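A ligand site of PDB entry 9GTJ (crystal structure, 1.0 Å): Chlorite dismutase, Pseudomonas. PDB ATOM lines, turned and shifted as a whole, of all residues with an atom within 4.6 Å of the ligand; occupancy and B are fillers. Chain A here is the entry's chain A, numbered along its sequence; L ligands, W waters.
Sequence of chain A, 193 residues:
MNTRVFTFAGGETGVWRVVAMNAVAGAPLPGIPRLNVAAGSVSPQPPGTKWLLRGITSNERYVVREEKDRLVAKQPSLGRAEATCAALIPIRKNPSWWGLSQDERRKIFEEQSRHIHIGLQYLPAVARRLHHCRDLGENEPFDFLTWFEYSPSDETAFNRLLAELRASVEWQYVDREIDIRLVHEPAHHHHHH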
ATOM      1  N   ASN A  59       0.953   6.616  34.838  1.00  0.00           N
ATOM      2  CA  ASN A  59       0.020   7.263  33.920  1.00  0.00           C
ATOM      3  C   ASN A  59       0.760   7.732  32.673  1.00  0.00           C
ATOM      4  O   ASN A  59       1.972   7.973  32.661  1.00  0.00           O
ATOM      5  CB  ASN A  59      -0.709   8.419  34.593  1.00  0.00           C
ATOM      6  CG  ASN A  59       0.254   9.460  35.139  1.00  0.00           C
ATOM      7  OD1 ASN A  59       0.828   9.285  36.200  1.00  0.00           O
ATOM      8  ND2 ASN A  59       0.398  10.566  34.411  1.00  0.00           N
ATOM      9  N   GLU A  60      -0.030   7.950  31.633  1.00  0.00           N
ATOM     10  CA  GLU A  60       0.475   8.488  30.381  1.00  0.00           C
ATOM     11  C   GLU A  60       0.993   9.907  30.591  1.00  0.00           C
ATOM     12  O   GLU A  60       0.395  10.720  31.301  1.00  0.00           O
ATOM     13  CB  GLU A  60      -0.630   8.492  29.323  1.00  0.00           C
ATOM     14  CG  GLU A  60      -0.984   7.066  28.908  1.00  0.00           C
ATOM     15  CD  GLU A  60      -2.421   6.841  28.506  1.00  0.00           C
ATOM     16  OE1 GLU A  60      -3.276   7.654  28.883  1.00  0.00           O
ATOM     17  OE2 GLU A  60      -2.661   5.815  27.861  1.00  0.00           O
ATOM     18  N   ARG A  61       2.112  10.187  29.905  1.00  0.00           N
ATOM     19  CA  ARG A  61       2.775  11.470  29.959  1.00  0.00           C
ATOM     20  C   ARG A  61       2.648  12.256  28.660  1.00  0.00           C
ATOM     21  O   ARG A  61       2.870  13.459  28.663  1.00  0.00           O
ATOM     22  CB  ARG A  61       4.260  11.251  30.260  1.00  0.00           C
ATOM     23  CG  ARG A  61       4.526  10.371  31.477  1.00  0.00           C
ATOM     24  CD  ARG A  61       3.826  10.891  32.750  1.00  0.00           C
ATOM     25  NE  ARG A  61       3.969   9.945  33.848  1.00  0.00           N
ATOM     26  CZ  ARG A  61       5.056   9.898  34.620  1.00  0.00           C
ATOM     27  NH1 ARG A  61       6.057  10.756  34.391  1.00  0.00           N
ATOM     28  NH2 ARG A  61       5.243   8.973  35.570  1.00  0.00           N
ATOM     29  N   TYR A  62       2.320  11.565  27.566  1.00  0.00           N
ATOM     30  CA  TYR A  62       2.347  12.172  26.232  1.00  0.00           C
ATOM     31  C   TYR A  62       1.147  11.793  25.373  1.00  0.00           C
ATOM     32  O   TYR A  62       0.668  12.620  24.600  1.00  0.00           O
ATOM     33  CB  TYR A  62       3.628  11.810  25.449  1.00  0.00           C
ATOM     34  CG  TYR A  62       4.880  12.336  26.125  1.00  0.00           C
ATOM     35  CD1 TYR A  62       5.118  13.700  26.210  1.00  0.00           C
ATOM     36  CD2 TYR A  62       5.767  11.482  26.745  1.00  0.00           C
ATOM     37  CE1 TYR A  62       6.208  14.187  26.921  1.00  0.00           C
ATOM     38  CE2 TYR A  62       6.859  11.946  27.452  1.00  0.00           C
ATOM     39  CZ  TYR A  62       7.089  13.306  27.551  1.00  0.00           C
ATOM     40  OH  TYR A  62       8.125  13.827  28.265  1.00  0.00           O
ATOM     41  N   VAL A  63       0.685  10.551  25.447  1.00  0.00           N
ATOM     42  CA  VAL A  63      -0.266  10.075  24.478  1.00  0.00           C
ATOM     43  C   VAL A  63      -1.595  10.828  24.642  1.00  0.00           C
ATOM     44  O   VAL A  63      -2.089  11.144  25.732  1.00  0.00           O
ATOM     45  CB  VAL A  63      -0.381   8.544  24.591  1.00  0.00           C
ATOM     46  CG1 VAL A  63      -1.091   8.131  25.856  1.00  0.00           C
ATOM     47  CG2 VAL A  63      -1.056   7.903  23.409  1.00  0.00           C
ATOM     48  N   LEU A  71      -3.918   2.501  20.009  1.00  0.00           N
ATOM     49  CA  LEU A  71      -3.082   1.576  20.753  1.00  0.00           C
ATOM     50  C   LEU A  71      -3.915   0.492  21.417  1.00  0.00           C
ATOM     51  O   LEU A  71      -3.560  -0.690  21.363  1.00  0.00           O
ATOM     52  CB  LEU A  71      -2.287   2.354  21.792  1.00  0.00           C
ATOM     53  CG  LEU A  71      -1.171   3.228  21.222  1.00  0.00           C
ATOM     54  CD1 LEU A  71      -0.748   4.273  22.236  1.00  0.00           C
ATOM     55  CD2 LEU A  71       0.038   2.411  20.829  1.00  0.00           C
ATOM     56  N   ILE A  89      14.987  -3.434  27.994  1.00  0.00           N
ATOM     57  CA  ILE A  89      15.801  -2.342  27.452  1.00  0.00           C
ATOM     58  C   ILE A  89      15.717  -1.184  28.454  1.00  0.00           C
ATOM     59  O   ILE A  89      14.833  -0.327  28.399  1.00  0.00           O
ATOM     60  CB  ILE A  89      15.378  -1.935  26.034  1.00  0.00           C
ATOM     61  CG1 ILE A  89      15.381  -3.166  25.110  1.00  0.00           C
ATOM     62  CG2 ILE A  89      16.294  -0.839  25.529  1.00  0.00           C
ATOM     63  CD1 ILE A  89      14.984  -2.882  23.672  1.00  0.00           C
ATOM     64  N   ILE A  91      16.763   2.395  29.753  1.00  0.00           N
ATOM     65  CA  ILE A  91      17.068   3.616  29.041  1.00  0.00           C
ATOM     66  C   ILE A  91      17.232   4.762  30.036  1.00  0.00           C
ATOM     67  O   ILE A  91      16.433   4.901  30.984  1.00  0.00           O
ATOM     68  CB  ILE A  91      15.951   3.960  28.035  1.00  0.00           C
ATOM     69  CG1 ILE A  91      16.029   2.932  26.914  1.00  0.00           C
ATOM     70  CG2 ILE A  91      16.028   5.403  27.537  1.00  0.00           C
ATOM     71  CD1 ILE A  91      14.944   2.933  25.917  1.00  0.00           C
ATOM     72  N   LYS A  93      17.701   9.092  29.928  1.00  0.00           N
ATOM     73  CA  LYS A  93      17.716  10.329  29.157  1.00  0.00           C
ATOM     74  C   LYS A  93      18.508  11.394  29.893  1.00  0.00           C
ATOM     75  O   LYS A  93      18.552  11.365  31.121  1.00  0.00           O
ATOM     76  CB  LYS A  93      16.290  10.804  28.841  1.00  0.00           C
ATOM     77  CG  LYS A  93      15.559   9.875  27.869  1.00  0.00           C
ATOM     78  CD  LYS A  93      14.184  10.373  27.445  1.00  0.00           C
ATOM     79  CE  LYS A  93      13.543   9.507  26.406  1.00  0.00           C
ATOM     80  NZ  LYS A  93      12.324  10.122  25.835  1.00  0.00           N
ATOM     81  N   TRP A  97      16.990  16.901  28.727  1.00  0.00           N
ATOM     82  CA  TRP A  97      15.650  16.419  28.450  1.00  0.00           C
ATOM     83  C   TRP A  97      14.705  16.737  29.606  1.00  0.00           C
ATOM     84  O   TRP A  97      13.624  17.276  29.417  1.00  0.00           O
ATOM     85  CB  TRP A  97      15.689  14.909  28.200  1.00  0.00           C
ATOM     86  CG  TRP A  97      14.327  14.294  28.072  1.00  0.00           C
ATOM     87  CD1 TRP A  97      13.614  13.643  29.037  1.00  0.00           C
ATOM     88  CD2 TRP A  97      13.476  14.326  26.916  1.00  0.00           C
ATOM     89  NE1 TRP A  97      12.414  13.224  28.550  1.00  0.00           N
ATOM     90  CE2 TRP A  97      12.281  13.651  27.255  1.00  0.00           C
ATOM     91  CE3 TRP A  97      13.598  14.868  25.634  1.00  0.00           C
ATOM     92  CZ2 TRP A  97      11.240  13.464  26.331  1.00  0.00           C
ATOM     93  CZ3 TRP A  97      12.566  14.699  24.734  1.00  0.00           C
ATOM     94  CH2 TRP A  97      11.418  13.996  25.081  1.00  0.00           C
ATOM     95  N   PHE A 109       8.992  13.960  21.100  1.00  0.00           N
ATOM     96  CA  PHE A 109       8.584  12.575  21.230  1.00  0.00           C
ATOM     97  C   PHE A 109       7.701  12.125  20.060  1.00  0.00           C
ATOM     98  O   PHE A 109       7.967  11.055  19.491  1.00  0.00           O
ATOM     99  CB  PHE A 109       7.844  12.426  22.565  1.00  0.00           C
ATOM    100  CG  PHE A 109       7.265  11.056  22.780  1.00  0.00           C
ATOM    101  CD1 PHE A 109       8.076  10.009  23.202  1.00  0.00           C
ATOM    102  CD2 PHE A 109       5.928  10.828  22.591  1.00  0.00           C
ATOM    103  CE1 PHE A 109       7.544   8.749  23.388  1.00  0.00           C
ATOM    104  CE2 PHE A 109       5.408   9.553  22.747  1.00  0.00           C
ATOM    105  CZ  PHE A 109       6.220   8.537  23.136  1.00  0.00           C
ATOM    106  N   HIS A 115       7.257   8.494  17.618  1.00  0.00           N
ATOM    107  CA  HIS A 115       7.437   7.273  18.397  1.00  0.00           C
ATOM    108  C   HIS A 115       6.218   6.365  18.298  1.00  0.00           C
ATOM    109  O   HIS A 115       6.343   5.163  18.041  1.00  0.00           O
ATOM    110  CB  HIS A 115       7.719   7.664  19.845  1.00  0.00           C
ATOM    111  CG  HIS A 115       8.083   6.531  20.752  1.00  0.00           C
ATOM    112  ND1 HIS A 115       9.272   6.554  21.452  1.00  0.00           N
ATOM    113  CD2 HIS A 115       7.449   5.448  21.221  1.00  0.00           C
ATOM    114  CE1 HIS A 115       9.307   5.508  22.264  1.00  0.00           C
ATOM    115  NE2 HIS A 115       8.219   4.789  22.132  1.00  0.00           N
ATOM    116  N   ILE A 116       5.038   6.915  18.556  1.00  0.00           N
ATOM    117  CA  ILE A 116       3.806   6.112  18.578  1.00  0.00           C
ATOM    118  C   ILE A 116       3.435   5.645  17.168  1.00  0.00           C
ATOM    119  O   ILE A 116       3.067   4.500  16.957  1.00  0.00           O
ATOM    120  CB  ILE A 116       2.668   6.896  19.257  1.00  0.00           C
ATOM    121  CG1 ILE A 116       3.025   7.250  20.707  1.00  0.00           C
ATOM    122  CG2 ILE A 116       1.381   6.115  19.166  1.00  0.00           C
ATOM    123  CD1 ILE A 116       2.093   8.262  21.353  1.00  0.00           C
ATOM    124  N   GLY A 119       5.764   2.869  16.445  1.00  0.00           N
ATOM    125  CA  GLY A 119       5.490   1.679  17.225  1.00  0.00           C
ATOM    126  C   GLY A 119       4.230   0.941  16.785  1.00  0.00           C
ATOM    127  O   GLY A 119       4.202  -0.276  16.769  1.00  0.00           O
ATOM    128  N   LEU A 120       3.195   1.702  16.378  1.00  0.00           N
ATOM    129  CA  LEU A 120       1.938   1.079  15.954  1.00  0.00           C
ATOM    130  C   LEU A 120       2.167   0.137  14.774  1.00  0.00           C
ATOM    131  O   LEU A 120       1.367  -0.792  14.572  1.00  0.00           O
ATOM    132  CB  LEU A 120       0.954   2.171  15.551  1.00  0.00           C
ATOM    133  CG  LEU A 120       0.185   2.772  16.717  1.00  0.00           C
ATOM    134  CD1 LEU A 120      -0.432   4.083  16.317  1.00  0.00           C
ATOM    135  CD2 LEU A 120      -0.904   1.833  17.247  1.00  0.00           C
ATOM    136  N   LEU A 123       2.655  -3.586  15.850  1.00  0.00           N
ATOM    137  CA  LEU A 123       1.583  -4.245  16.575  1.00  0.00           C
ATOM    138  C   LEU A 123       0.754  -4.945  15.519  1.00  0.00           C
ATOM    139  O   LEU A 123       0.537  -4.419  14.430  1.00  0.00           O
ATOM    140  CB  LEU A 123       0.730  -3.205  17.331  1.00  0.00           C
ATOM    141  CG  LEU A 123       1.283  -2.775  18.693  1.00  0.00           C
ATOM    142  CD1 LEU A 123       2.758  -2.587  18.826  1.00  0.00           C
ATOM    143  CD2 LEU A 123       0.503  -1.567  19.167  1.00  0.00           C
ATOM    144  N   VAL A 126       4.419  -7.075  18.597  1.00  0.00           N
ATOM    145  CA  VAL A 126       5.220  -6.770  19.773  1.00  0.00           C
ATOM    146  C   VAL A 126       4.316  -6.294  20.908  1.00  0.00           C
ATOM    147  O   VAL A 126       3.580  -5.305  20.768  1.00  0.00           O
ATOM    148  CB  VAL A 126       6.263  -5.700  19.439  1.00  0.00           C
ATOM    149  CG1 VAL A 126       7.118  -5.339  20.647  1.00  0.00           C
ATOM    150  CG2 VAL A 126       7.153  -6.110  18.297  1.00  0.00           C
ATOM    151  N   ARG A 128       4.270  -4.830  24.898  1.00  0.00           N
ATOM    152  CA  ARG A 128       5.162  -3.886  25.551  1.00  0.00           C
ATOM    153  C   ARG A 128       4.663  -3.506  26.937  1.00  0.00           C
ATOM    154  O   ARG A 128       3.458  -3.524  27.186  1.00  0.00           O
ATOM    155  CB  ARG A 128       5.332  -2.612  24.705  1.00  0.00           C
ATOM    156  CG  ARG A 128       4.132  -1.682  24.719  1.00  0.00           C
ATOM    157  CD  ARG A 128       4.168  -0.579  23.673  1.00  0.00           C
ATOM    158  NE  ARG A 128       3.176   0.470  23.908  1.00  0.00           N
ATOM    159  CZ  ARG A 128       1.862   0.300  23.824  1.00  0.00           C
ATOM    160  NH1 ARG A 128       1.352  -0.754  23.184  1.00  0.00           N
ATOM    161  NH2 ARG A 128       1.043   1.220  24.296  1.00  0.00           N
ATOM    162  N   LEU A 130       5.945  -0.287  29.786  1.00  0.00           N
ATOM    163  CA  LEU A 130       6.804   0.813  30.176  1.00  0.00           C
ATOM    164  C   LEU A 130       6.842   0.965  31.693  1.00  0.00           C
ATOM    165  O   LEU A 130       5.788   1.058  32.333  1.00  0.00           O
ATOM    166  CB  LEU A 130       6.278   2.094  29.556  1.00  0.00           C
ATOM    167  CG  LEU A 130       6.997   3.394  29.905  1.00  0.00           C
ATOM    168  CD1 LEU A 130       8.451   3.376  29.450  1.00  0.00           C
ATOM    169  CD2 LEU A 130       6.239   4.581  29.313  1.00  0.00           C
ATOM    170  N   PHE A 144      14.014   4.570  32.588  1.00  0.00           N
ATOM    171  CA  PHE A 144      12.933   3.712  32.163  1.00  0.00           C
ATOM    172  C   PHE A 144      13.437   2.297  32.072  1.00  0.00           C
ATOM    173  O   PHE A 144      14.577   2.056  31.688  1.00  0.00           O
ATOM    174  CB  PHE A 144      12.399   4.105  30.789  1.00  0.00           C
ATOM    175  CG  PHE A 144      11.998   5.554  30.689  1.00  0.00           C
ATOM    176  CD1 PHE A 144      10.782   5.985  31.181  1.00  0.00           C
ATOM    177  CD2 PHE A 144      12.848   6.460  30.113  1.00  0.00           C
ATOM    178  CE1 PHE A 144      10.444   7.327  31.067  1.00  0.00           C
ATOM    179  CE2 PHE A 144      12.499   7.790  30.017  1.00  0.00           C
ATOM    180  CZ  PHE A 144      11.302   8.222  30.493  1.00  0.00           C
ATOM    181  N   THR A 146      12.074  -0.704  29.814  1.00  0.00           N
ATOM    182  CA  THR A 146      11.103  -1.060  28.777  1.00  0.00           C
ATOM    183  C   THR A 146      11.173  -2.560  28.569  1.00  0.00           C
ATOM    184  O   THR A 146      12.252  -3.147  28.579  1.00  0.00           O
ATOM    185  CB  THR A 146      11.294  -0.208  27.513  1.00  0.00           C
ATOM    186  OG1 THR A 146      12.504  -0.513  26.838  1.00  0.00           O
ATOM    187  CG2 THR A 146      11.172   1.281  27.803  1.00  0.00           C
ATOM    188  N   PHE A 148       9.485  -5.945  26.330  1.00  0.00           N
ATOM    189  CA  PHE A 148       8.811  -6.329  25.104  1.00  0.00           C
ATOM    190  C   PHE A 148       8.750  -7.849  25.025  1.00  0.00           C
ATOM    191  O   PHE A 148       9.647  -8.537  25.488  1.00  0.00           O
ATOM    192  CB  PHE A 148       9.574  -5.797  23.894  1.00  0.00           C
ATOM    193  CG  PHE A 148       9.792  -4.319  23.979  1.00  0.00           C
ATOM    194  CD1 PHE A 148       8.784  -3.442  23.601  1.00  0.00           C
ATOM    195  CD2 PHE A 148      10.948  -3.805  24.543  1.00  0.00           C
ATOM    196  CE1 PHE A 148       8.924  -2.082  23.790  1.00  0.00           C
ATOM    197  CE2 PHE A 148      11.100  -2.445  24.740  1.00  0.00           C
ATOM    198  CZ  PHE A 148      10.090  -1.577  24.366  1.00  0.00           C
ATOM    199  N   PHE A 158      11.262  -6.741  15.221  1.00  0.00           N
ATOM    200  CA  PHE A 158      11.592  -5.995  16.427  1.00  0.00           C
ATOM    201  C   PHE A 158      12.909  -5.234  16.234  1.00  0.00           C
ATOM    202  O   PHE A 158      13.050  -4.088  16.658  1.00  0.00           O
ATOM    203  CB  PHE A 158      11.667  -6.943  17.620  1.00  0.00           C
ATOM    204  CG  PHE A 158      11.945  -6.257  18.926  1.00  0.00           C
ATOM    205  CD1 PHE A 158      10.983  -5.454  19.497  1.00  0.00           C
ATOM    206  CD2 PHE A 158      13.151  -6.408  19.582  1.00  0.00           C
ATOM    207  CE1 PHE A 158      11.201  -4.806  20.700  1.00  0.00           C
ATOM    208  CE2 PHE A 158      13.369  -5.760  20.785  1.00  0.00           C
ATOM    209  CZ  PHE A 158      12.401  -4.973  21.342  1.00  0.00           C
ATOM    210  N   LEU A 161      12.271  -2.153  14.283  1.00  0.00           N
ATOM    211  CA  LEU A 161      11.683  -1.131  15.139  1.00  0.00           C
ATOM    212  C   LEU A 161      12.757  -0.403  15.924  1.00  0.00           C
ATOM    213  O   LEU A 161      12.765   0.825  15.986  1.00  0.00           O
ATOM    214  CB  LEU A 161      10.664  -1.806  16.073  1.00  0.00           C
ATOM    215  CG  LEU A 161      10.195  -1.021  17.281  1.00  0.00           C
ATOM    216  CD1 LEU A 161       9.472   0.262  16.920  1.00  0.00           C
ATOM    217  CD2 LEU A 161       9.334  -1.919  18.151  1.00  0.00           C
ATOM    218  N   LEU A 162      13.651  -1.166  16.555  1.00  0.00           N
ATOM    219  CA  LEU A 162      14.701  -0.536  17.358  1.00  0.00           C
ATOM    220  C   LEU A 162      15.525   0.415  16.492  1.00  0.00           C
ATOM    221  O   LEU A 162      15.888   1.512  16.939  1.00  0.00           O
ATOM    222  CB  LEU A 162      15.619  -1.576  17.967  1.00  0.00           C
ATOM    223  CG  LEU A 162      14.945  -2.449  19.029  1.00  0.00           C
ATOM    224  CD1 LEU A 162      15.886  -3.542  19.433  1.00  0.00           C
ATOM    225  CD2 LEU A 162      14.515  -1.626  20.215  1.00  0.00           C
ATOM    226  N   LEU A 165      13.602   3.717  15.961  1.00  0.00           N
ATOM    227  CA  LEU A 165      13.573   4.597  17.119  1.00  0.00           C
ATOM    228  C   LEU A 165      14.961   5.171  17.406  1.00  0.00           C
ATOM    229  O   LEU A 165      15.098   6.358  17.740  1.00  0.00           O
ATOM    230  CB  LEU A 165      13.038   3.865  18.336  1.00  0.00           C
ATOM    231  CG  LEU A 165      11.558   3.456  18.225  1.00  0.00           C
ATOM    232  CD1 LEU A 165      11.158   2.690  19.483  1.00  0.00           C
ATOM    233  CD2 LEU A 165      10.644   4.650  18.063  1.00  0.00           C
ATOM    234  N   GLU A 170      14.268  11.930  19.331  1.00  0.00           N
ATOM    235  CA  GLU A 170      14.129  11.587  20.746  1.00  0.00           C
ATOM    236  C   GLU A 170      15.410  10.926  21.261  1.00  0.00           C
ATOM    237  O   GLU A 170      15.845  11.162  22.372  1.00  0.00           O
ATOM    238  CB  GLU A 170      12.929  10.652  20.924  1.00  0.00           C
ATOM    239  CG  GLU A 170      12.711  10.173  22.341  1.00  0.00           C
ATOM    240  CD  GLU A 170      11.615   9.140  22.491  1.00  0.00           C
ATOM    241  OE1 GLU A 170      10.997   8.703  21.497  1.00  0.00           O
ATOM    242  OE2 GLU A 170      11.374   8.732  23.662  1.00  0.00           O
ATOM    243  N   TRP A 171      16.003  10.055  20.430  1.00  0.00           N
ATOM    244  CA  TRP A 171      17.159   9.298  20.858  1.00  0.00           C
ATOM    245  C   TRP A 171      18.439  10.134  20.943  1.00  0.00           C
ATOM    246  O   TRP A 171      19.433   9.688  21.516  1.00  0.00           O
ATOM    247  CB  TRP A 171      17.369   8.057  19.992  1.00  0.00           C
ATOM    248  CG  TRP A 171      17.042   6.784  20.727  1.00  0.00           C
ATOM    249  CD1 TRP A 171      17.940   5.876  21.188  1.00  0.00           C
ATOM    250  CD2 TRP A 171      15.747   6.316  21.120  1.00  0.00           C
ATOM    251  NE1 TRP A 171      17.298   4.871  21.851  1.00  0.00           N
ATOM    252  CE2 TRP A 171      15.958   5.108  21.810  1.00  0.00           C
ATOM    253  CE3 TRP A 171      14.438   6.786  20.939  1.00  0.00           C
ATOM    254  CZ2 TRP A 171      14.900   4.341  22.296  1.00  0.00           C
ATOM    255  CZ3 TRP A 171      13.386   6.035  21.439  1.00  0.00           C
ATOM    256  CH2 TRP A 171      13.625   4.825  22.112  1.00  0.00           C
ATOM    257  N   GLU A 177      21.642   3.054  27.169  1.00  0.00           N
ATOM    258  CA  GLU A 177      20.701   2.074  26.651  1.00  0.00           C
ATOM    259  C   GLU A 177      21.406   0.734  26.634  1.00  0.00           C
ATOM    260  O   GLU A 177      22.487   0.605  26.086  1.00  0.00           O
ATOM    261  CB  GLU A 177      20.187   2.471  25.270  1.00  0.00           C
ATOM    262  CG  GLU A 177      19.239   1.440  24.673  1.00  0.00           C
ATOM    263  CD  GLU A 177      18.590   1.839  23.361  1.00  0.00           C
ATOM    264  OE1 GLU A 177      18.956   2.887  22.800  1.00  0.00           O
ATOM    265  OE2 GLU A 177      17.716   1.085  22.868  1.00  0.00           O
HETATM  266  C1  LIG L   1       6.987   5.747  25.672  1.00  0.00           C
HETATM  267  C2  LIG L   1       4.449   3.305  22.393  1.00  0.00           C
HETATM  268  C3  LIG L   1       8.319   0.632  21.400  1.00  0.00           C
HETATM  269  C4  LIG L   1      10.910   3.181  24.563  1.00  0.00           C
HETATM  270  C5  LIG L   1       5.969   5.314  24.859  1.00  0.00           C
HETATM  271  C6  LIG L   1       4.613   5.879  24.864  1.00  0.00           C
HETATM  272  C7  LIG L   1       3.878   5.148  23.978  1.00  0.00           C
HETATM  273  C8  LIG L   1       4.797   4.211  23.377  1.00  0.00           C
HETATM  274  C9  LIG L   1       2.405   5.278  23.705  1.00  0.00           C
HETATM  275  C10 LIG L   1       4.126   7.116  25.653  1.00  0.00           C
HETATM  276  C11 LIG L   1       3.574   6.676  26.906  1.00  0.00           C
HETATM  277  C12 LIG L   1       3.117   7.968  27.657  1.00  0.00           C
HETATM  278  O1  LIG L   1       3.555   8.147  28.819  1.00  0.00           O
HETATM  279  O2  LIG L   1       2.285   8.785  27.112  1.00  0.00           O
HETATM  280  C13 LIG L   1       5.299   2.384  21.794  1.00  0.00           C
HETATM  281  C14 LIG L   1       4.852   1.383  20.879  1.00  0.00           C
HETATM  282  C15 LIG L   1       5.921   0.563  20.655  1.00  0.00           C
HETATM  283  C16 LIG L   1       7.028   1.115  21.427  1.00  0.00           C
HETATM  284  C17 LIG L   1       3.443   1.277  20.320  1.00  0.00           C
HETATM  285  C18 LIG L   1       5.916  -0.680  19.891  1.00  0.00           C
HETATM  286  C19 LIG L   1       6.500  -1.802  20.224  1.00  0.00           C
HETATM  287  C20 LIG L   1       9.404   1.122  22.144  1.00  0.00           C
HETATM  288  C21 LIG L   1      10.718   0.582  22.097  1.00  0.00           C
HETATM  289  C22 LIG L   1      11.474   1.317  22.976  1.00  0.00           C
HETATM  290  C23 LIG L   1      10.567   2.303  23.569  1.00  0.00           C
HETATM  291  C24 LIG L   1      11.143  -0.590  21.271  1.00  0.00           C
HETATM  292  C25 LIG L   1      12.885   1.158  23.363  1.00  0.00           C
HETATM  293  C26 LIG L   1      13.858   0.923  22.542  1.00  0.00           C
HETATM  294  C27 LIG L   1      10.066   4.070  25.194  1.00  0.00           C
HETATM  295  C28 LIG L   1      10.469   5.014  26.248  1.00  0.00           C
HETATM  296  C29 LIG L   1       9.354   5.721  26.577  1.00  0.00           C
HETATM  297  C30 LIG L   1       8.280   5.240  25.697  1.00  0.00           C
HETATM  298  C31 LIG L   1      11.843   5.108  26.810  1.00  0.00           C
HETATM  299  C32 LIG L   1       9.212   6.817  27.583  1.00  0.00           C
HETATM  300  C33 LIG L   1       9.370   8.177  26.950  1.00  0.00           C
HETATM  301  C34 LIG L   1       9.434   9.302  27.946  1.00  0.00           C
HETATM  302  O3  LIG L   1       8.564   9.336  28.840  1.00  0.00           O
HETATM  303  O4  LIG L   1      10.302  10.218  27.765  1.00  0.00           O
HETATM  304  N1  LIG L   1       6.060   4.325  23.929  1.00  0.00           N
HETATM  305  N2  LIG L   1       6.600   2.212  22.116  1.00  0.00           N
HETATM  306  N3  LIG L   1       9.323   2.163  23.043  1.00  0.00           N
HETATM  307  N4  LIG L   1       8.746   4.247  24.875  1.00  0.00           N
HETATM  308 FE1  LIG L   1       7.699   3.300  23.438  1.00  0.00          FE
HETATM  309  O   HOH W   1       2.816   2.704  25.903  1.00  0.00           O
HETATM  310  O   HOH W   2       1.587   4.320  27.642  1.00  0.00           O
HETATM  311  O   HOH W   3      13.566   6.982  24.576  1.00  0.00           O
HETATM  312  O   HOH W   4       6.292   8.110  29.564  1.00  0.00           O
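Merely in contact with the ligand: Phe 148, Phe 144, Leu 165, Arg 128, Glu 60, Leu 161, Leu 162, Phe 109, Trp 171, Gly 119, Val 126, Leu 71, Ile 116, Trp 97, Ile 91, Thr 146, Leu 130, Leu 123, Glu 177, Glu 170 and Leu 120.
Within 4 Å of the ligand: Glu 60, Arg 61, Tyr 62, Val 63, Leu 71, Ile 91, Lys 93, Trp 97, Phe 109, His 115, Ile 116, Gly 119, Leu 120, Leu 123, Val 126, Arg 128, Leu 130, Phe 144, Thr 146, Phe 148, Leu 161, Leu 162, Leu 165, Glu 170, Trp 171 and Glu 177.
Along chain A the residues within 4 Å of the ligand span positions 60 to 177.
O of Phe 109 is in hydrogen-bond range of N of His 115, 3.3 Å away.
OE1 of Glu 170 sits at hydrogen-bond distance from ND1 of His 115.
The backbone carbonyl oxygen (O) of Asn 59 is in hydrogen-bond range of the guanidinium group (NE) of Arg 61 (3.0 Å).
The side-chain amino group (NZ) of Lys 93 lies within salt-bridge range of the side-chain carboxylate (OE2) of Glu 170 (2.7 Å).
The backbone NH (N) of Phe 144 is in hydrogen-bond range of the backbone carbonyl oxygen (O) of Ile 91 (2.9 Å).
The indole nitrogen of Trp 171 lies within hydrogen-bond range of the side-chain carboxylate of Glu 177 (2.8 Å).
The backbone carbonyl oxygen of Ile 89 lies within hydrogen-bond range of the side-chain hydroxyl of Thr 146 (2.8 Å).
FE1 of the ligand is bound by NE2 of His 115.
The backbone NH (N) of Arg 61 sits at hydrogen-bond distance from an oxygen (O1) of the ligand (2.7 Å).
NZ of Lys 93 lies within salt-bridge range of O4 of the ligand, at 2.8 Å.
The backbone NH of Tyr 62 sits at hydrogen-bond distance from an oxygen (O2) of the ligand.
O2 of the ligand sits at hydrogen-bond distance from N of Val 63 (2.9 Å).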
